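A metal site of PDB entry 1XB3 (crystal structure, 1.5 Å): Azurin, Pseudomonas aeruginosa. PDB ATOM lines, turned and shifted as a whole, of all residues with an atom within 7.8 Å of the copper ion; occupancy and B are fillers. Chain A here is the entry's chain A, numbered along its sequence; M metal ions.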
ATOM      1  N   GLY A   9       2.278 -14.913 -23.686  1.00  0.00           N
ATOM      2  CA  GLY A   9       1.884 -16.160 -24.366  1.00  0.00           C
ATOM      3  C   GLY A   9       2.690 -16.227 -25.637  1.00  0.00           C
ATOM      4  O   GLY A   9       2.661 -15.292 -26.404  1.00  0.00           O
ATOM      5  N   ASN A  10       3.376 -17.337 -25.909  1.00  0.00           N
ATOM      6  CA  ASN A  10       4.329 -17.376 -27.011  1.00  0.00           C
ATOM      7  C   ASN A  10       3.916 -18.342 -28.122  1.00  0.00           C
ATOM      8  O   ASN A  10       2.818 -18.903 -28.096  1.00  0.00           O
ATOM      9  CB  ASN A  10       5.744 -17.671 -26.501  1.00  0.00           C
ATOM     10  CG  ASN A  10       5.897 -19.071 -25.920  1.00  0.00           C
ATOM     11  OD1 ASN A  10       5.051 -19.942 -26.102  1.00  0.00           O
ATOM     12  ND2 ASN A  10       6.989 -19.310 -25.240  1.00  0.00           N
ATOM     13  N   MET A  13       2.976 -22.144 -27.301  1.00  0.00           N
ATOM     14  CA  MET A  13       1.819 -22.538 -26.506  1.00  0.00           C
ATOM     15  C   MET A  13       2.070 -22.445 -25.007  1.00  0.00           C
ATOM     16  O   MET A  13       1.490 -23.211 -24.210  1.00  0.00           O
ATOM     17  CB  MET A  13       1.392 -23.976 -26.874  1.00  0.00           C
ATOM     18  CG  MET A  13      -0.074 -24.215 -26.710  1.00  0.00           C
ATOM     19  SD  MET A  13      -0.990 -23.194 -27.856  1.00  0.00           S
ATOM     20  CE  MET A  13      -0.808 -24.118 -29.379  1.00  0.00           C
ATOM     21  N   GLN A  14       2.916 -21.490 -24.596  1.00  0.00           N
ATOM     22  CA  GLN A  14       3.263 -21.373 -23.177  1.00  0.00           C
ATOM     23  C   GLN A  14       2.881 -19.990 -22.658  1.00  0.00           C
ATOM     24  O   GLN A  14       3.195 -18.980 -23.296  1.00  0.00           O
ATOM     25  CB  GLN A  14       4.789 -21.498 -22.979  1.00  0.00           C
ATOM     26  CG  GLN A  14       5.404 -22.863 -23.369  1.00  0.00           C
ATOM     27  CD  GLN A  14       6.919 -22.829 -23.672  1.00  0.00           C
ATOM     28  OE1 GLN A  14       7.544 -21.779 -23.861  1.00  0.00           O
ATOM     29  NE2 GLN A  14       7.511 -24.012 -23.724  1.00  0.00           N
ATOM     30  N   PHE A  15       2.240 -19.965 -21.497  1.00  0.00           N
ATOM     31  CA  PHE A  15       2.232 -18.756 -20.656  1.00  0.00           C
ATOM     32  C   PHE A  15       3.519 -18.822 -19.828  1.00  0.00           C
ATOM     33  O   PHE A  15       4.048 -19.915 -19.540  1.00  0.00           O
ATOM     34  CB  PHE A  15       1.062 -18.719 -19.674  1.00  0.00           C
ATOM     35  CG  PHE A  15      -0.282 -18.294 -20.256  1.00  0.00           C
ATOM     36  CD1 PHE A  15      -1.389 -19.061 -19.958  1.00  0.00           C
ATOM     37  CD2 PHE A  15      -0.448 -17.135 -20.984  1.00  0.00           C
ATOM     38  CE1 PHE A  15      -2.657 -18.688 -20.389  1.00  0.00           C
ATOM     39  CE2 PHE A  15      -1.687 -16.756 -21.435  1.00  0.00           C
ATOM     40  CZ  PHE A  15      -2.802 -17.535 -21.137  1.00  0.00           C
ATOM     41  N   HIS A  35       2.427 -10.941 -26.518  1.00  0.00           N
ATOM     42  CA  HIS A  35       2.634 -12.122 -27.349  1.00  0.00           C
ATOM     43  C   HIS A  35       3.957 -11.985 -28.082  1.00  0.00           C
ATOM     44  O   HIS A  35       3.993 -11.438 -29.187  1.00  0.00           O
ATOM     45  CB  HIS A  35       1.468 -12.254 -28.316  1.00  0.00           C
ATOM     46  CG  HIS A  35       1.399 -13.564 -29.036  1.00  0.00           C
ATOM     47  ND1 HIS A  35       2.510 -14.230 -29.532  1.00  0.00           N
ATOM     48  CD2 HIS A  35       0.315 -14.309 -29.388  1.00  0.00           C
ATOM     49  CE1 HIS A  35       2.111 -15.332 -30.143  1.00  0.00           C
ATOM     50  NE2 HIS A  35       0.782 -15.414 -30.070  1.00  0.00           N
ATOM     51  N   LYS A  41      -2.791 -14.038 -34.915  1.00  0.00           N
ATOM     52  CA  LYS A  41      -3.787 -14.495 -33.960  1.00  0.00           C
ATOM     53  C   LYS A  41      -4.774 -15.588 -34.460  1.00  0.00           C
ATOM     54  O   LYS A  41      -5.395 -16.272 -33.643  1.00  0.00           O
ATOM     55  CB  LYS A  41      -4.540 -13.317 -33.358  1.00  0.00           C
ATOM     56  CG  LYS A  41      -5.549 -12.708 -34.191  1.00  0.00           C
ATOM     57  CD  LYS A  41      -6.232 -11.563 -33.439  1.00  0.00           C
ATOM     58  CE  LYS A  41      -7.188 -10.879 -34.313  1.00  0.00           C
ATOM     59  NZ  LYS A  41      -7.767  -9.740 -33.591  1.00  0.00           N
ATOM     60  N   VAL A  43      -3.785 -18.188 -36.021  1.00  0.00           N
ATOM     61  CA  VAL A  43      -3.014 -19.428 -35.903  1.00  0.00           C
ATOM     62  C   VAL A  43      -2.583 -19.733 -34.461  1.00  0.00           C
ATOM     63  O   VAL A  43      -2.512 -20.886 -34.042  1.00  0.00           O
ATOM     64  CB  VAL A  43      -1.735 -19.323 -36.776  1.00  0.00           C
ATOM     65  CG1 VAL A  43      -0.783 -20.456 -36.518  1.00  0.00           C
ATOM     66  CG2 VAL A  43      -2.142 -19.281 -38.245  1.00  0.00           C
ATOM     67  N   MET A  44      -2.233 -18.682 -33.740  1.00  0.00           N
ATOM     68  CA  MET A  44      -1.646 -18.826 -32.390  1.00  0.00           C
ATOM     69  C   MET A  44      -2.123 -17.680 -31.498  1.00  0.00           C
ATOM     70  O   MET A  44      -1.364 -17.156 -30.703  1.00  0.00           O
ATOM     71  CB  MET A  44      -0.114 -18.859 -32.512  1.00  0.00           C
ATOM     72  CG  MET A  44       0.639 -19.261 -31.320  1.00  0.00           C
ATOM     73  SD  MET A  44       0.295 -20.897 -30.696  1.00  0.00           S
ATOM     74  CE  MET A  44       0.771 -21.964 -32.079  1.00  0.00           C
ATOM     75  N   GLY A  45      -3.374 -17.291 -31.649  1.00  0.00           N
ATOM     76  CA  GLY A  45      -3.957 -16.255 -30.786  1.00  0.00           C
ATOM     77  C   GLY A  45      -4.002 -16.677 -29.332  1.00  0.00           C
ATOM     78  O   GLY A  45      -4.215 -17.851 -29.013  1.00  0.00           O
ATOM     79  N   HIS A  46      -3.773 -15.717 -28.440  1.00  0.00           N
ATOM     80  CA  HIS A  46      -3.912 -15.968 -27.018  1.00  0.00           C
ATOM     81  C   HIS A  46      -4.740 -14.901 -26.355  1.00  0.00           C
ATOM     82  O   HIS A  46      -4.627 -13.701 -26.685  1.00  0.00           O
ATOM     83  CB  HIS A  46      -2.560 -16.009 -26.300  1.00  0.00           C
ATOM     84  CG  HIS A  46      -1.602 -17.012 -26.854  1.00  0.00           C
ATOM     85  ND1 HIS A  46      -1.889 -18.351 -27.003  1.00  0.00           N
ATOM     86  CD2 HIS A  46      -0.290 -16.864 -27.147  1.00  0.00           C
ATOM     87  CE1 HIS A  46      -0.811 -18.963 -27.460  1.00  0.00           C
ATOM     88  NE2 HIS A  46       0.168 -18.093 -27.538  1.00  0.00           N
ATOM     89  N   ASN A  47      -5.550 -15.321 -25.390  1.00  0.00           N
ATOM     90  CA  ASN A  47      -6.170 -14.386 -24.457  1.00  0.00           C
ATOM     91  C   ASN A  47      -5.824 -14.846 -23.044  1.00  0.00           C
ATOM     92  O   ASN A  47      -5.197 -15.916 -22.866  1.00  0.00           O
ATOM     93  CB  ASN A  47      -7.693 -14.230 -24.735  1.00  0.00           C
ATOM     94  CG  ASN A  47      -8.452 -15.531 -24.754  1.00  0.00           C
ATOM     95  OD1 ASN A  47      -7.971 -16.552 -24.257  1.00  0.00           O
ATOM     96  ND2 ASN A  47      -9.719 -15.499 -25.312  1.00  0.00           N
ATOM     97  N   TRP A  48      -6.226 -14.042 -22.069  1.00  0.00           N
ATOM     98  CA  TRP A  48      -6.137 -14.381 -20.667  1.00  0.00           C
ATOM     99  C   TRP A  48      -7.559 -14.245 -20.105  1.00  0.00           C
ATOM    100  O   TRP A  48      -8.159 -13.158 -20.153  1.00  0.00           O
ATOM    101  CB  TRP A  48      -5.147 -13.460 -19.955  1.00  0.00           C
ATOM    102  CG  TRP A  48      -4.919 -13.816 -18.533  1.00  0.00           C
ATOM    103  CD1 TRP A  48      -3.923 -14.626 -18.028  1.00  0.00           C
ATOM    104  CD2 TRP A  48      -5.676 -13.367 -17.415  1.00  0.00           C
ATOM    105  NE1 TRP A  48      -4.043 -14.708 -16.657  1.00  0.00           N
ATOM    106  CE2 TRP A  48      -5.122 -13.963 -16.261  1.00  0.00           C
ATOM    107  CE3 TRP A  48      -6.780 -12.527 -17.270  1.00  0.00           C
ATOM    108  CZ2 TRP A  48      -5.656 -13.746 -15.002  1.00  0.00           C
ATOM    109  CZ3 TRP A  48      -7.316 -12.341 -16.010  1.00  0.00           C
ATOM    110  CH2 TRP A  48      -6.701 -12.891 -14.877  1.00  0.00           C
ATOM    111  N   LEU A  86      -8.257 -11.373 -27.577  1.00  0.00           N
ATOM    112  CA  LEU A  86      -7.358 -12.308 -28.241  1.00  0.00           C
ATOM    113  C   LEU A  86      -6.327 -11.492 -28.979  1.00  0.00           C
ATOM    114  O   LEU A  86      -6.668 -10.583 -29.746  1.00  0.00           O
ATOM    115  CB  LEU A  86      -8.132 -13.188 -29.203  1.00  0.00           C
ATOM    116  CG  LEU A  86      -7.432 -14.440 -29.704  1.00  0.00           C
ATOM    117  CD1 LEU A  86      -7.404 -15.579 -28.695  1.00  0.00           C
ATOM    118  CD2 LEU A  86      -8.032 -14.866 -31.040  1.00  0.00           C
ATOM    119  N   ILE A  87      -5.061 -11.815 -28.749  1.00  0.00           N
ATOM    120  CA  ILE A  87      -3.967 -11.126 -29.406  1.00  0.00           C
ATOM    121  C   ILE A  87      -3.053 -12.080 -30.170  1.00  0.00           C
ATOM    122  O   ILE A  87      -2.921 -13.230 -29.851  1.00  0.00           O
ATOM    123  CB  ILE A  87      -3.129 -10.334 -28.414  1.00  0.00           C
ATOM    124  CG1 ILE A  87      -2.477 -11.247 -27.397  1.00  0.00           C
ATOM    125  CG2 ILE A  87      -3.997  -9.236 -27.781  1.00  0.00           C
ATOM    126  CD1 ILE A  87      -1.475 -10.538 -26.515  1.00  0.00           C
ATOM    127  N   PHE A 111      -6.673 -19.080 -18.109  1.00  0.00           N
ATOM    128  CA  PHE A 111      -6.453 -19.900 -19.293  1.00  0.00           C
ATOM    129  C   PHE A 111      -6.670 -19.087 -20.549  1.00  0.00           C
ATOM    130  O   PHE A 111      -7.240 -17.991 -20.506  1.00  0.00           O
ATOM    131  CB  PHE A 111      -7.411 -21.105 -19.262  1.00  0.00           C
ATOM    132  CG  PHE A 111      -8.836 -20.755 -18.892  1.00  0.00           C
ATOM    133  CD1 PHE A 111      -9.241 -20.681 -17.562  1.00  0.00           C
ATOM    134  CD2 PHE A 111      -9.744 -20.431 -19.873  1.00  0.00           C
ATOM    135  CE1 PHE A 111     -10.557 -20.356 -17.232  1.00  0.00           C
ATOM    136  CE2 PHE A 111     -11.043 -20.092 -19.564  1.00  0.00           C
ATOM    137  CZ  PHE A 111     -11.438 -20.056 -18.223  1.00  0.00           C
ATOM    138  N   CYS A 112      -6.166 -19.640 -21.655  1.00  0.00           N
ATOM    139  CA  CYS A 112      -6.448 -19.184 -23.018  1.00  0.00           C
ATOM    140  C   CYS A 112      -7.593 -20.018 -23.610  1.00  0.00           C
ATOM    141  O   CYS A 112      -7.583 -21.262 -23.470  1.00  0.00           O
ATOM    142  CB  CYS A 112      -5.208 -19.336 -23.879  1.00  0.00           C
ATOM    143  SG  CYS A 112      -5.530 -18.769 -25.553  1.00  0.00           S
ATOM    144  N   THR A 113      -8.554 -19.355 -24.264  1.00  0.00           N
ATOM    145  CA  THR A 113      -9.674 -20.080 -24.876  1.00  0.00           C
ATOM    146  C   THR A 113      -9.529 -20.313 -26.375  1.00  0.00           C
ATOM    147  O   THR A 113     -10.443 -20.833 -26.999  1.00  0.00           O
ATOM    148  CB  THR A 113     -11.004 -19.408 -24.589  1.00  0.00           C
ATOM    149  OG1 THR A 113     -11.029 -18.110 -25.189  1.00  0.00           O
ATOM    150  CG2 THR A 113     -11.273 -19.299 -23.090  1.00  0.00           C
ATOM    151  N   PHE A 114      -8.402 -19.966 -26.969  1.00  0.00           N
ATOM    152  CA  PHE A 114      -8.191 -20.336 -28.387  1.00  0.00           C
ATOM    153  C   PHE A 114      -8.306 -21.870 -28.484  1.00  0.00           C
ATOM    154  O   PHE A 114      -7.777 -22.577 -27.620  1.00  0.00           O
ATOM    155  CB  PHE A 114      -6.821 -19.845 -28.853  1.00  0.00           C
ATOM    156  CG  PHE A 114      -6.566 -20.020 -30.332  1.00  0.00           C
ATOM    157  CD1 PHE A 114      -6.643 -18.933 -31.200  1.00  0.00           C
ATOM    158  CD2 PHE A 114      -6.303 -21.257 -30.863  1.00  0.00           C
ATOM    159  CE1 PHE A 114      -6.418 -19.072 -32.560  1.00  0.00           C
ATOM    160  CE2 PHE A 114      -6.075 -21.406 -32.252  1.00  0.00           C
ATOM    161  CZ  PHE A 114      -6.120 -20.321 -33.090  1.00  0.00           C
ATOM    162  N   PRO A 115      -9.005 -22.390 -29.499  1.00  0.00           N
ATOM    163  CA  PRO A 115      -9.260 -23.814 -29.518  1.00  0.00           C
ATOM    164  C   PRO A 115      -8.041 -24.695 -29.293  1.00  0.00           C
ATOM    165  O   PRO A 115      -7.024 -24.613 -30.005  1.00  0.00           O
ATOM    166  CB  PRO A 115      -9.854 -24.054 -30.925  1.00  0.00           C
ATOM    167  CG  PRO A 115     -10.502 -22.775 -31.274  1.00  0.00           C
ATOM    168  CD  PRO A 115      -9.621 -21.707 -30.664  1.00  0.00           C
ATOM    169  N   GLY A 116      -8.160 -25.530 -28.256  1.00  0.00           N
ATOM    170  CA  GLY A 116      -7.123 -26.466 -27.860  1.00  0.00           C
ATOM    171  C   GLY A 116      -6.017 -25.927 -26.966  1.00  0.00           C
ATOM    172  O   GLY A 116      -5.283 -26.678 -26.352  1.00  0.00           O
ATOM    173  N   HIS A 117      -5.910 -24.612 -26.837  1.00  0.00           N
ATOM    174  CA  HIS A 117      -4.765 -24.065 -26.063  1.00  0.00           C
ATOM    175  C   HIS A 117      -4.768 -24.363 -24.581  1.00  0.00           C
ATOM    176  O   HIS A 117      -3.696 -24.526 -24.001  1.00  0.00           O
ATOM    177  CB  HIS A 117      -4.646 -22.553 -26.275  1.00  0.00           C
ATOM    178  CG  HIS A 117      -4.112 -22.194 -27.629  1.00  0.00           C
ATOM    179  ND1 HIS A 117      -3.588 -20.943 -27.920  1.00  0.00           N
ATOM    180  CD2 HIS A 117      -3.974 -22.930 -28.753  1.00  0.00           C
ATOM    181  CE1 HIS A 117      -3.207 -20.920 -29.190  1.00  0.00           C
ATOM    182  NE2 HIS A 117      -3.404 -22.126 -29.711  1.00  0.00           N
ATOM    183  N   SER A 118      -5.961 -24.449 -23.978  1.00  0.00           N
ATOM    184  CA  SER A 118      -6.053 -24.512 -22.507  1.00  0.00           C
ATOM    185  C   SER A 118      -5.446 -25.789 -21.928  1.00  0.00           C
ATOM    186  O   SER A 118      -5.238 -25.863 -20.728  1.00  0.00           O
ATOM    187  CB  SER A 118      -7.476 -24.377 -22.026  1.00  0.00           C
ATOM    188  OG  SER A 118      -8.247 -25.508 -22.386  1.00  0.00           O
ATOM    189  N   MET A 121      -2.104 -23.929 -21.698  1.00  0.00           N
ATOM    190  CA  MET A 121      -2.113 -22.517 -21.319  1.00  0.00           C
ATOM    191  C   MET A 121      -3.188 -22.322 -20.229  1.00  0.00           C
ATOM    192  O   MET A 121      -4.335 -21.938 -20.480  1.00  0.00           O
ATOM    193  CB  MET A 121      -2.332 -21.653 -22.546  1.00  0.00           C
ATOM    194  CG  MET A 121      -1.269 -21.840 -23.566  1.00  0.00           C
ATOM    195  SD  MET A 121      -1.317 -20.667 -24.905  1.00  0.00           S
ATOM    196  CE  MET A 121      -0.721 -19.194 -24.018  1.00  0.00           C
HETATM  197 CU    CU M   1      -3.685 -19.289 -26.752  1.00  0.00          CU
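Residues that only touch the copper ion: Met 121 (3.3 Å) and Phe 114 (3.8 Å).
The nearest printed residue that does not touch the copper ion is Asn 47 (4.6 Å).
The copper ion is bound by ND1 of His 117 (2.0 Å), ND1 of His 46 (2.0 Å) and SG of Cys 112 (2.3 Å).
The copper ion has three donor atoms within binding distance.
Slightly farther from the copper ion lies the backbone carbonyl oxygen (O) of Gly 45 (2.7 Å).
O of Asn 10 lies within hydrogen-bond range of NE2 of His 46, at 2.8 Å.
The side-chain sulfur (SD) of Met 121 sits close to a ring nitrogen (ND1) of His 46 (3.2 Å).
The backbone NH (N) of Phe 114 sits close to the side-chain sulfur (SG) of Cys 112 (3.4 Å).
A ring nitrogen (NE2) of His 117 lies close to the side-chain sulfur (SD) of Met 13 (3.2 Å).
A ring nitrogen (ND1) of His 117 sits close to the backbone carbonyl oxygen of Gly 45 (3.3 Å).
A ring nitrogen (ND1) of His 117 lies close to the side-chain sulfur (SD) of Met 121, at 3.8 Å.
The backbone NH of Cys 112 lies within hydrogen-bond range of the backbone carbonyl oxygen of Met 121 (3.2 Å).
The backbone carbonyl oxygen of His 46 is in hydrogen-bond range of the backbone NH of Ile 87 (2.8 Å).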
